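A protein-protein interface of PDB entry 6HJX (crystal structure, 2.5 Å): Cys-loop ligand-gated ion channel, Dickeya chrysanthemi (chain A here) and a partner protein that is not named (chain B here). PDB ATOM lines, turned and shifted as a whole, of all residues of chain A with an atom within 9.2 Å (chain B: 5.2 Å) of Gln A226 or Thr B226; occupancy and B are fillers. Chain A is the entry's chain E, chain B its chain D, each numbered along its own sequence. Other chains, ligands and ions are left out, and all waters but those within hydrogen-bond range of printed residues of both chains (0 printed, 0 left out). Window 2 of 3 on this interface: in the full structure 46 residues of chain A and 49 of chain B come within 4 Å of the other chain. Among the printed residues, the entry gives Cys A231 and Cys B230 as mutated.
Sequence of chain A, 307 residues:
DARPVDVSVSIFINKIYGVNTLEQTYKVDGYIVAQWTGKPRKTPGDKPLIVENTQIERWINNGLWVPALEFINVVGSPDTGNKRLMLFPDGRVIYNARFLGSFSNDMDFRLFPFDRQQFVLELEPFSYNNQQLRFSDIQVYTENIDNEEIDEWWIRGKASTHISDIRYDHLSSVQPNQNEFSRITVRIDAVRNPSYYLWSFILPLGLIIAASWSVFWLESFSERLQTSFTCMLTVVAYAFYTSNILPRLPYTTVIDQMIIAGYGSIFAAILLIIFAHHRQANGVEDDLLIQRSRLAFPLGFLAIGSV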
ATOM      1  N   VAL A 215       2.860   5.842  -9.069  1.00  0.00           N
ATOM      2  CA  VAL A 215       2.666   4.726  -8.148  1.00  0.00           C
ATOM      3  C   VAL A 215       3.334   3.469  -8.690  1.00  0.00           C
ATOM      4  O   VAL A 215       3.794   2.617  -7.920  1.00  0.00           O
ATOM      5  CB  VAL A 215       1.163   4.492  -7.884  1.00  0.00           C
ATOM      6  CG1 VAL A 215       0.564   5.675  -7.135  1.00  0.00           C
ATOM      7  CG2 VAL A 215       0.413   4.238  -9.187  1.00  0.00           C
ATOM      8  N   LEU A 218       6.886   2.924  -7.186  1.00  0.00           N
ATOM      9  CA  LEU A 218       7.101   2.421  -5.838  1.00  0.00           C
ATOM     10  C   LEU A 218       7.294   0.910  -5.891  1.00  0.00           C
ATOM     11  O   LEU A 218       6.659   0.215  -6.688  1.00  0.00           O
ATOM     12  CB  LEU A 218       5.921   2.788  -4.940  1.00  0.00           C
ATOM     13  CG  LEU A 218       5.725   4.292  -4.724  1.00  0.00           C
ATOM     14  CD1 LEU A 218       4.297   4.593  -4.300  1.00  0.00           C
ATOM     15  CD2 LEU A 218       6.711   4.819  -3.691  1.00  0.00           C
ATOM     16  N   SER A 220       7.256  -1.599  -3.290  1.00  0.00           N
ATOM     17  CA  SER A 220       6.457  -2.526  -2.500  1.00  0.00           C
ATOM     18  C   SER A 220       4.975  -2.339  -2.807  1.00  0.00           C
ATOM     19  O   SER A 220       4.520  -1.234  -3.113  1.00  0.00           O
ATOM     20  CB  SER A 220       6.701  -2.332  -1.003  1.00  0.00           C
ATOM     21  OG  SER A 220       5.877  -1.306  -0.481  1.00  0.00           O
ATOM     22  N   PHE A 221       4.224  -3.438  -2.714  1.00  0.00           N
ATOM     23  CA  PHE A 221       2.796  -3.390  -3.008  1.00  0.00           C
ATOM     24  C   PHE A 221       2.047  -2.511  -2.013  1.00  0.00           C
ATOM     25  O   PHE A 221       1.121  -1.786  -2.392  1.00  0.00           O
ATOM     26  CB  PHE A 221       2.219  -4.806  -3.015  1.00  0.00           C
ATOM     27  CG  PHE A 221       0.752  -4.868  -2.696  1.00  0.00           C
ATOM     28  CD1 PHE A 221      -0.197  -4.563  -3.658  1.00  0.00           C
ATOM     29  CD2 PHE A 221       0.321  -5.240  -1.432  1.00  0.00           C
ATOM     30  CE1 PHE A 221      -1.548  -4.622  -3.364  1.00  0.00           C
ATOM     31  CE2 PHE A 221      -1.026  -5.304  -1.133  1.00  0.00           C
ATOM     32  CZ  PHE A 221      -1.962  -4.994  -2.100  1.00  0.00           C
ATOM     33  N   SER A 222       2.428  -2.563  -0.735  1.00  0.00           N
ATOM     34  CA  SER A 222       1.766  -1.732   0.263  1.00  0.00           C
ATOM     35  C   SER A 222       1.998  -0.248   0.017  1.00  0.00           C
ATOM     36  O   SER A 222       1.221   0.578   0.506  1.00  0.00           O
ATOM     37  CB  SER A 222       2.247  -2.111   1.664  1.00  0.00           C
ATOM     38  OG  SER A 222       3.651  -1.964   1.775  1.00  0.00           O
ATOM     39  N   GLU A 223       3.045   0.108  -0.730  1.00  0.00           N
ATOM     40  CA  GLU A 223       3.301   1.511  -1.032  1.00  0.00           C
ATOM     41  C   GLU A 223       2.483   1.983  -2.227  1.00  0.00           C
ATOM     42  O   GLU A 223       1.948   3.097  -2.213  1.00  0.00           O
ATOM     43  CB  GLU A 223       4.792   1.727  -1.289  1.00  0.00           C
ATOM     44  CG  GLU A 223       5.646   1.640  -0.036  1.00  0.00           C
ATOM     45  CD  GLU A 223       7.126   1.526  -0.344  1.00  0.00           C
ATOM     46  OE1 GLU A 223       7.502   1.646  -1.530  1.00  0.00           O
ATOM     47  OE2 GLU A 223       7.912   1.315   0.604  1.00  0.00           O
ATOM     48  N   ARG A 224       2.374   1.154  -3.268  1.00  0.00           N
ATOM     49  CA  ARG A 224       1.615   1.547  -4.449  1.00  0.00           C
ATOM     50  C   ARG A 224       0.163   1.842  -4.092  1.00  0.00           C
ATOM     51  O   ARG A 224      -0.398   2.864  -4.502  1.00  0.00           O
ATOM     52  CB  ARG A 224       1.685   0.446  -5.510  1.00  0.00           C
ATOM     53  CG  ARG A 224       3.088  -0.048  -5.820  1.00  0.00           C
ATOM     54  CD  ARG A 224       3.095  -1.019  -6.995  1.00  0.00           C
ATOM     55  NE  ARG A 224       4.307  -1.837  -7.017  1.00  0.00           N
ATOM     56  CZ  ARG A 224       4.381  -3.102  -6.605  1.00  0.00           C
ATOM     57  NH1 ARG A 224       3.310  -3.733  -6.139  1.00  0.00           N
ATOM     58  NH2 ARG A 224       5.538  -3.746  -6.669  1.00  0.00           N
ATOM     59  N   LEU A 225      -0.461   0.949  -3.320  1.00  0.00           N
ATOM     60  CA  LEU A 225      -1.886   1.068  -3.038  1.00  0.00           C
ATOM     61  C   LEU A 225      -2.183   2.207  -2.071  1.00  0.00           C
ATOM     62  O   LEU A 225      -3.243   2.835  -2.168  1.00  0.00           O
ATOM     63  CB  LEU A 225      -2.408  -0.258  -2.481  1.00  0.00           C
ATOM     64  CG  LEU A 225      -3.893  -0.354  -2.130  1.00  0.00           C
ATOM     65  CD1 LEU A 225      -4.765   0.106  -3.285  1.00  0.00           C
ATOM     66  CD2 LEU A 225      -4.232  -1.784  -1.746  1.00  0.00           C
ATOM     67  N   GLN A 226      -1.269   2.495  -1.145  1.00  0.00           N
ATOM     68  CA  GLN A 226      -1.513   3.542  -0.159  1.00  0.00           C
ATOM     69  C   GLN A 226      -1.251   4.935  -0.718  1.00  0.00           C
ATOM     70  O   GLN A 226      -1.951   5.886  -0.351  1.00  0.00           O
ATOM     71  CB  GLN A 226      -0.657   3.288   1.082  1.00  0.00           C
ATOM     72  CG  GLN A 226      -1.067   2.031   1.841  1.00  0.00           C
ATOM     73  CD  GLN A 226      -0.189   1.752   3.043  1.00  0.00           C
ATOM     74  OE1 GLN A 226       1.032   1.895   2.984  1.00  0.00           O
ATOM     75  NE2 GLN A 226      -0.811   1.353   4.147  1.00  0.00           N
ATOM     76  N   THR A 227      -0.258   5.087  -1.599  1.00  0.00           N
ATOM     77  CA  THR A 227      -0.082   6.362  -2.285  1.00  0.00           C
ATOM     78  C   THR A 227      -1.229   6.631  -3.251  1.00  0.00           C
ATOM     79  O   THR A 227      -1.508   7.793  -3.568  1.00  0.00           O
ATOM     80  CB  THR A 227       1.252   6.388  -3.034  1.00  0.00           C
ATOM     81  OG1 THR A 227       2.323   6.108  -2.123  1.00  0.00           O
ATOM     82  CG2 THR A 227       1.487   7.754  -3.674  1.00  0.00           C
ATOM     83  N   SER A 228      -1.901   5.578  -3.723  1.00  0.00           N
ATOM     84  CA  SER A 228      -3.043   5.766  -4.607  1.00  0.00           C
ATOM     85  C   SER A 228      -4.171   6.504  -3.900  1.00  0.00           C
ATOM     86  O   SER A 228      -4.878   7.310  -4.517  1.00  0.00           O
ATOM     87  CB  SER A 228      -3.533   4.415  -5.127  1.00  0.00           C
ATOM     88  OG  SER A 228      -2.563   3.807  -5.960  1.00  0.00           O
ATOM     89  N   PHE A 229      -4.363   6.240  -2.605  1.00  0.00           N
ATOM     90  CA  PHE A 229      -5.373   6.976  -1.852  1.00  0.00           C
ATOM     91  C   PHE A 229      -4.963   8.430  -1.662  1.00  0.00           C
ATOM     92  O   PHE A 229      -5.807   9.331  -1.728  1.00  0.00           O
ATOM     93  CB  PHE A 229      -5.620   6.304  -0.504  1.00  0.00           C
ATOM     94  CG  PHE A 229      -6.299   4.973  -0.613  1.00  0.00           C
ATOM     95  CD1 PHE A 229      -7.656   4.895  -0.878  1.00  0.00           C
ATOM     96  CD2 PHE A 229      -5.583   3.800  -0.457  1.00  0.00           C
ATOM     97  CE1 PHE A 229      -8.286   3.672  -0.983  1.00  0.00           C
ATOM     98  CE2 PHE A 229      -6.207   2.572  -0.561  1.00  0.00           C
ATOM     99  CZ  PHE A 229      -7.560   2.508  -0.824  1.00  0.00           C
ATOM    100  N   THR A 230      -3.674   8.683  -1.423  1.00  0.00           N
ATOM    101  CA  THR A 230      -3.199  10.062  -1.388  1.00  0.00           C
ATOM    102  C   THR A 230      -3.501  10.767  -2.705  1.00  0.00           C
ATOM    103  O   THR A 230      -3.879  11.945  -2.715  1.00  0.00           O
ATOM    104  CB  THR A 230      -1.700  10.098  -1.090  1.00  0.00           C
ATOM    105  OG1 THR A 230      -1.440   9.449   0.160  1.00  0.00           O
ATOM    106  CG2 THR A 230      -1.197  11.535  -1.019  1.00  0.00           C
ATOM    107  N   CYS A 231      -3.351  10.055  -3.825  1.00  0.00           N
ATOM    108  CA  CYS A 231      -3.663  10.633  -5.129  1.00  0.00           C
ATOM    109  C   CYS A 231      -5.164  10.824  -5.299  1.00  0.00           C
ATOM    110  O   CYS A 231      -5.622  11.901  -5.698  1.00  0.00           O
ATOM    111  CB  CYS A 231      -3.111   9.746  -6.245  1.00  0.00           C
ATOM    112  SG  CYS A 231      -1.321   9.576  -6.228  1.00  0.00           S
ATOM    113  N   MET A 232      -5.946   9.777  -5.023  1.00  0.00           N
ATOM    114  CA  MET A 232      -7.399   9.907  -5.014  1.00  0.00           C
ATOM    115  C   MET A 232      -7.832  11.116  -4.194  1.00  0.00           C
ATOM    116  O   MET A 232      -8.707  11.883  -4.612  1.00  0.00           O
ATOM    117  CB  MET A 232      -8.028   8.631  -4.449  1.00  0.00           C
ATOM    118  CG  MET A 232      -9.550   8.621  -4.446  1.00  0.00           C
ATOM    119  SD  MET A 232     -10.235   8.361  -6.091  1.00  0.00           S
ATOM    120  CE  MET A 232      -9.932   6.610  -6.308  1.00  0.00           C
ATOM    121  N   LEU A 233      -7.225  11.301  -3.020  1.00  0.00           N
ATOM    122  CA  LEU A 233      -7.592  12.415  -2.152  1.00  0.00           C
ATOM    123  C   LEU A 233      -7.169  13.752  -2.751  1.00  0.00           C
ATOM    124  O   LEU A 233      -7.782  14.787  -2.454  1.00  0.00           O
ATOM    125  CB  LEU A 233      -6.963  12.207  -0.772  1.00  0.00           C
ATOM    126  CG  LEU A 233      -7.568  12.889   0.457  1.00  0.00           C
ATOM    127  CD1 LEU A 233      -9.057  12.635   0.560  1.00  0.00           C
ATOM    128  CD2 LEU A 233      -6.865  12.380   1.712  1.00  0.00           C
ATOM    129  N   ILE A 266      -6.820   6.675 -11.393  1.00  0.00           N
ATOM    130  CA  ILE A 266      -6.394   6.237 -10.068  1.00  0.00           C
ATOM    131  C   ILE A 266      -7.107   4.950  -9.679  1.00  0.00           C
ATOM    132  O   ILE A 266      -6.503   4.037  -9.103  1.00  0.00           O
ATOM    133  CB  ILE A 266      -6.636   7.358  -9.039  1.00  0.00           C
ATOM    134  CG1 ILE A 266      -5.734   8.555  -9.353  1.00  0.00           C
ATOM    135  CG2 ILE A 266      -6.398   6.851  -7.620  1.00  0.00           C
ATOM    136  CD1 ILE A 266      -6.050   9.802  -8.543  1.00  0.00           C
ATOM    137  N   ILE A 270      -5.462   1.254  -9.016  1.00  0.00           N
ATOM    138  CA  ILE A 270      -5.665   0.503  -7.782  1.00  0.00           C
ATOM    139  C   ILE A 270      -6.035  -0.942  -8.086  1.00  0.00           C
ATOM    140  O   ILE A 270      -5.669  -1.856  -7.337  1.00  0.00           O
ATOM    141  CB  ILE A 270      -6.733   1.196  -6.907  1.00  0.00           C
ATOM    142  CG1 ILE A 270      -6.141   2.459  -6.275  1.00  0.00           C
ATOM    143  CG2 ILE A 270      -7.265   0.240  -5.834  1.00  0.00           C
ATOM    144  CD1 ILE A 270      -7.131   3.291  -5.489  1.00  0.00           C
ATOM    145  N   ILE A 273      -2.858  -2.802  -9.359  1.00  0.00           N
ATOM    146  CA  ILE A 273      -1.893  -3.042  -8.290  1.00  0.00           C
ATOM    147  C   ILE A 273      -2.258  -4.300  -7.512  1.00  0.00           C
ATOM    148  O   ILE A 273      -1.382  -5.069  -7.101  1.00  0.00           O
ATOM    149  CB  ILE A 273      -1.806  -1.810  -7.370  1.00  0.00           C
ATOM    150  CG1 ILE A 273      -1.181  -0.635  -8.121  1.00  0.00           C
ATOM    151  CG2 ILE A 273      -0.992  -2.117  -6.118  1.00  0.00           C
ATOM    152  CD1 ILE A 273      -1.404   0.706  -7.452  1.00  0.00           C
ATOM    153  N   ILE A 274      -3.554  -4.527  -7.288  1.00  0.00           N
ATOM    154  CA  ILE A 274      -3.988  -5.695  -6.532  1.00  0.00           C
ATOM    155  C   ILE A 274      -3.977  -6.936  -7.414  1.00  0.00           C
ATOM    156  O   ILE A 274      -3.487  -7.998  -7.014  1.00  0.00           O
ATOM    157  CB  ILE A 274      -5.380  -5.447  -5.921  1.00  0.00           C
ATOM    158  CG1 ILE A 274      -5.353  -4.205  -5.028  1.00  0.00           C
ATOM    159  CG2 ILE A 274      -5.838  -6.662  -5.120  1.00  0.00           C
ATOM    160  CD1 ILE A 274      -6.725  -3.713  -4.630  1.00  0.00           C
ATOM    161  N   VAL B 214      -8.970  -2.093   1.300  1.00  0.00           N
ATOM    162  CA  VAL B 214      -8.228  -2.344   2.532  1.00  0.00           C
ATOM    163  C   VAL B 214      -8.163  -3.833   2.833  1.00  0.00           C
ATOM    164  O   VAL B 214      -7.196  -4.312   3.437  1.00  0.00           O
ATOM    165  CB  VAL B 214      -8.859  -1.566   3.706  1.00  0.00           C
ATOM    166  CG1 VAL B 214      -8.679  -0.073   3.504  1.00  0.00           C
ATOM    167  CG2 VAL B 214     -10.335  -1.926   3.863  1.00  0.00           C
ATOM    168  N   SER B 221      -2.044  -3.712  10.583  1.00  0.00           N
ATOM    169  CA  SER B 221      -1.606  -2.323  10.650  1.00  0.00           C
ATOM    170  C   SER B 221      -2.025  -1.559   9.398  1.00  0.00           C
ATOM    171  O   SER B 221      -2.612  -0.474   9.487  1.00  0.00           O
ATOM    172  CB  SER B 221      -0.090  -2.274  10.834  1.00  0.00           C
ATOM    173  OG  SER B 221       0.324  -1.037  11.381  1.00  0.00           O
ATOM    174  N   GLU B 222      -1.730  -2.117   8.221  1.00  0.00           N
ATOM    175  CA  GLU B 222      -2.074  -1.454   6.967  1.00  0.00           C
ATOM    176  C   GLU B 222      -3.579  -1.266   6.833  1.00  0.00           C
ATOM    177  O   GLU B 222      -4.048  -0.188   6.444  1.00  0.00           O
ATOM    178  CB  GLU B 222      -1.533  -2.265   5.786  1.00  0.00           C
ATOM    179  CG  GLU B 222      -0.167  -1.818   5.295  1.00  0.00           C
ATOM    180  CD  GLU B 222       0.732  -2.982   4.935  1.00  0.00           C
ATOM    181  OE1 GLU B 222       0.269  -3.899   4.226  1.00  0.00           O
ATOM    182  OE2 GLU B 222       1.902  -2.985   5.371  1.00  0.00           O
ATOM    183  N   ARG B 223      -4.354  -2.303   7.150  1.00  0.00           N
ATOM    184  CA  ARG B 223      -5.791  -2.261   6.896  1.00  0.00           C
ATOM    185  C   ARG B 223      -6.467  -1.186   7.737  1.00  0.00           C
ATOM    186  O   ARG B 223      -7.287  -0.411   7.232  1.00  0.00           O
ATOM    187  CB  ARG B 223      -6.411  -3.631   7.172  1.00  0.00           C
ATOM    188  CG  ARG B 223      -5.766  -4.759   6.381  1.00  0.00           C
ATOM    189  CD  ARG B 223      -6.603  -6.030   6.400  1.00  0.00           C
ATOM    190  NE  ARG B 223      -6.252  -6.917   7.507  1.00  0.00           N
ATOM    191  CZ  ARG B 223      -5.212  -7.747   7.501  1.00  0.00           C
ATOM    192  NH1 ARG B 223      -4.405  -7.804   6.450  1.00  0.00           N
ATOM    193  NH2 ARG B 223      -4.974  -8.519   8.552  1.00  0.00           N
ATOM    194  N   LEU B 224      -6.131  -1.122   9.028  1.00  0.00           N
ATOM    195  CA  LEU B 224      -6.805  -0.178   9.913  1.00  0.00           C
ATOM    196  C   LEU B 224      -6.382   1.256   9.621  1.00  0.00           C
ATOM    197  O   LEU B 224      -7.226   2.159   9.579  1.00  0.00           O
ATOM    198  CB  LEU B 224      -6.521  -0.537  11.370  1.00  0.00           C
ATOM    199  CG  LEU B 224      -7.258   0.296  12.418  1.00  0.00           C
ATOM    200  CD1 LEU B 224      -8.764   0.122  12.292  1.00  0.00           C
ATOM    201  CD2 LEU B 224      -6.789  -0.078  13.812  1.00  0.00           C
ATOM    202  N   GLN B 225      -5.086   1.489   9.410  1.00  0.00           N
ATOM    203  CA  GLN B 225      -4.617   2.844   9.137  1.00  0.00           C
ATOM    204  C   GLN B 225      -5.246   3.394   7.862  1.00  0.00           C
ATOM    205  O   GLN B 225      -5.711   4.539   7.830  1.00  0.00           O
ATOM    206  CB  GLN B 225      -3.091   2.866   9.040  1.00  0.00           C
ATOM    207  CG  GLN B 225      -2.381   2.770  10.384  1.00  0.00           C
ATOM    208  CD  GLN B 225      -0.911   3.129  10.291  1.00  0.00           C
ATOM    209  OE1 GLN B 225      -0.179   2.591   9.460  1.00  0.00           O
ATOM    210  NE2 GLN B 225      -0.474   4.052  11.140  1.00  0.00           N
ATOM    211  N   THR B 226      -5.274   2.589   6.798  1.00  0.00           N
ATOM    212  CA  THR B 226      -5.826   3.051   5.529  1.00  0.00           C
ATOM    213  C   THR B 226      -7.327   3.298   5.609  1.00  0.00           C
ATOM    214  O   THR B 226      -7.860   4.062   4.799  1.00  0.00           O
ATOM    215  CB  THR B 226      -5.517   2.036   4.422  1.00  0.00           C
ATOM    216  OG1 THR B 226      -4.100   1.842   4.335  1.00  0.00           O
ATOM    217  CG2 THR B 226      -6.033   2.518   3.068  1.00  0.00           C
ATOM    218  N   SER B 227      -8.021   2.677   6.566  1.00  0.00           N
ATOM    219  CA  SER B 227      -9.447   2.943   6.719  1.00  0.00           C
ATOM    220  C   SER B 227      -9.708   4.402   7.069  1.00  0.00           C
ATOM    221  O   SER B 227     -10.758   4.947   6.709  1.00  0.00           O
ATOM    222  CB  SER B 227     -10.045   2.028   7.789  1.00  0.00           C
ATOM    223  OG  SER B 227     -10.175   0.702   7.308  1.00  0.00           O
ATOM    224  N   PHE B 228      -8.773   5.051   7.767  1.00  0.00           N
ATOM    225  CA  PHE B 228      -8.950   6.459   8.104  1.00  0.00           C
ATOM    226  C   PHE B 228      -8.753   7.348   6.883  1.00  0.00           C
ATOM    227  O   PHE B 228      -9.486   8.325   6.697  1.00  0.00           O
ATOM    228  CB  PHE B 228      -7.989   6.861   9.221  1.00  0.00           C
ATOM    229  CG  PHE B 228      -8.397   6.362  10.573  1.00  0.00           C
ATOM    230  CD1 PHE B 228      -9.489   6.909  11.226  1.00  0.00           C
ATOM    231  CD2 PHE B 228      -7.688   5.348  11.194  1.00  0.00           C
ATOM    232  CE1 PHE B 228      -9.871   6.452  12.472  1.00  0.00           C
ATOM    233  CE2 PHE B 228      -8.063   4.889  12.440  1.00  0.00           C
ATOM    234  CZ  PHE B 228      -9.156   5.444  13.081  1.00  0.00           C
ATOM    235  N   THR B 229      -7.768   7.030   6.040  1.00  0.00           N
ATOM    236  CA  THR B 229      -7.614   7.773   4.797  1.00  0.00           C
ATOM    237  C   THR B 229      -8.870   7.678   3.941  1.00  0.00           C
ATOM    238  O   THR B 229      -9.200   8.622   3.215  1.00  0.00           O
ATOM    239  CB  THR B 229      -6.397   7.261   4.026  1.00  0.00           C
ATOM    240  OG1 THR B 229      -5.242   7.311   4.874  1.00  0.00           O
ATOM    241  CG2 THR B 229      -6.146   8.110   2.778  1.00  0.00           C
ATOM    242  N   CYS B 230      -9.588   6.554   4.020  1.00  0.00           N
ATOM    243  CA  CYS B 230     -10.840   6.415   3.283  1.00  0.00           C
ATOM    244  C   CYS B 230     -11.950   7.227   3.937  1.00  0.00           C
ATOM    245  O   CYS B 230     -12.653   7.990   3.264  1.00  0.00           O
ATOM    246  CB  CYS B 230     -11.236   4.940   3.197  1.00  0.00           C
ATOM    247  SG  CYS B 230     -10.140   3.925   2.175  1.00  0.00           S
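OG1 of Thr B226 lies within hydrogen-bond range of O of Glu B222, 2.9 Å away. The backbone carbonyl oxygen (O) of Thr B226 lies within hydrogen-bond range of the side-chain sulfur (SG) of Cys B230, at 3.5 Å. The side-chain hydroxyl (OG) of Ser A220 is in hydrogen-bond range of the side-chain hydroxyl (OG) of Ser A222 (3.2 Å). The backbone carbonyl oxygen (O) of Ser A222 sits close to the side-chain amide oxygen (OE1) of Gln A226.
The side-chain hydroxyl (OG1) of Thr B226 is in hydrogen-bond range of the side-chain amide nitrogen (NE2) of Gln A226, 3.3 Å away.
Glu B222 touches Ser A222 (OE1 to CB, 3.7 Å). NE2 of Gln A226 touches CG of Glu B222, at 3.4 Å. CE2 of Phe A229 touches CG2 of Thr B226, 3.6 Å away. Phe A229 touches Thr B229 (CB to CG2, 3.8 Å). SG of Cys B230 touches CE1 of Phe A229 (3.7 Å).
Of the printed residues of chain B, Ser A222 touches Glu B222 (3.7 Å). Gln A226 touches just these residues of chain B: Glu B222 and Thr B226. Thr A230 touches none of the printed residues of chain B. Of the printed residues of chain A, Glu B222 touches Ser A222 (3.7 Å) and Gln A226 (3.4 Å). Thr B226 touches just these residues of chain A: Gln A226 (3.3 Å) and Phe A229 (3.6 Å). No residue of chain A comes within 4 Å of Ser B227. Of chain A, only Phe A229 (3.8 Å) comes within 4 Å of Thr B229. Of the printed residues of chain A, Cys B230 touches Phe A229. The nearest residue of chain A that does not touch Thr B226 is Leu A225 (5.9 Å).
Of the 20 printed residues of chain A, 3 touch a printed residue of chain B. Hydrophobic or aromatic side chains of chain A within 4 Å of the printed part of chain B: Phe A229. Among the printed residues, no Asp or Glu carboxylate lies within 4 Å of a Lys or Arg side-chain nitrogen of the other chain.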
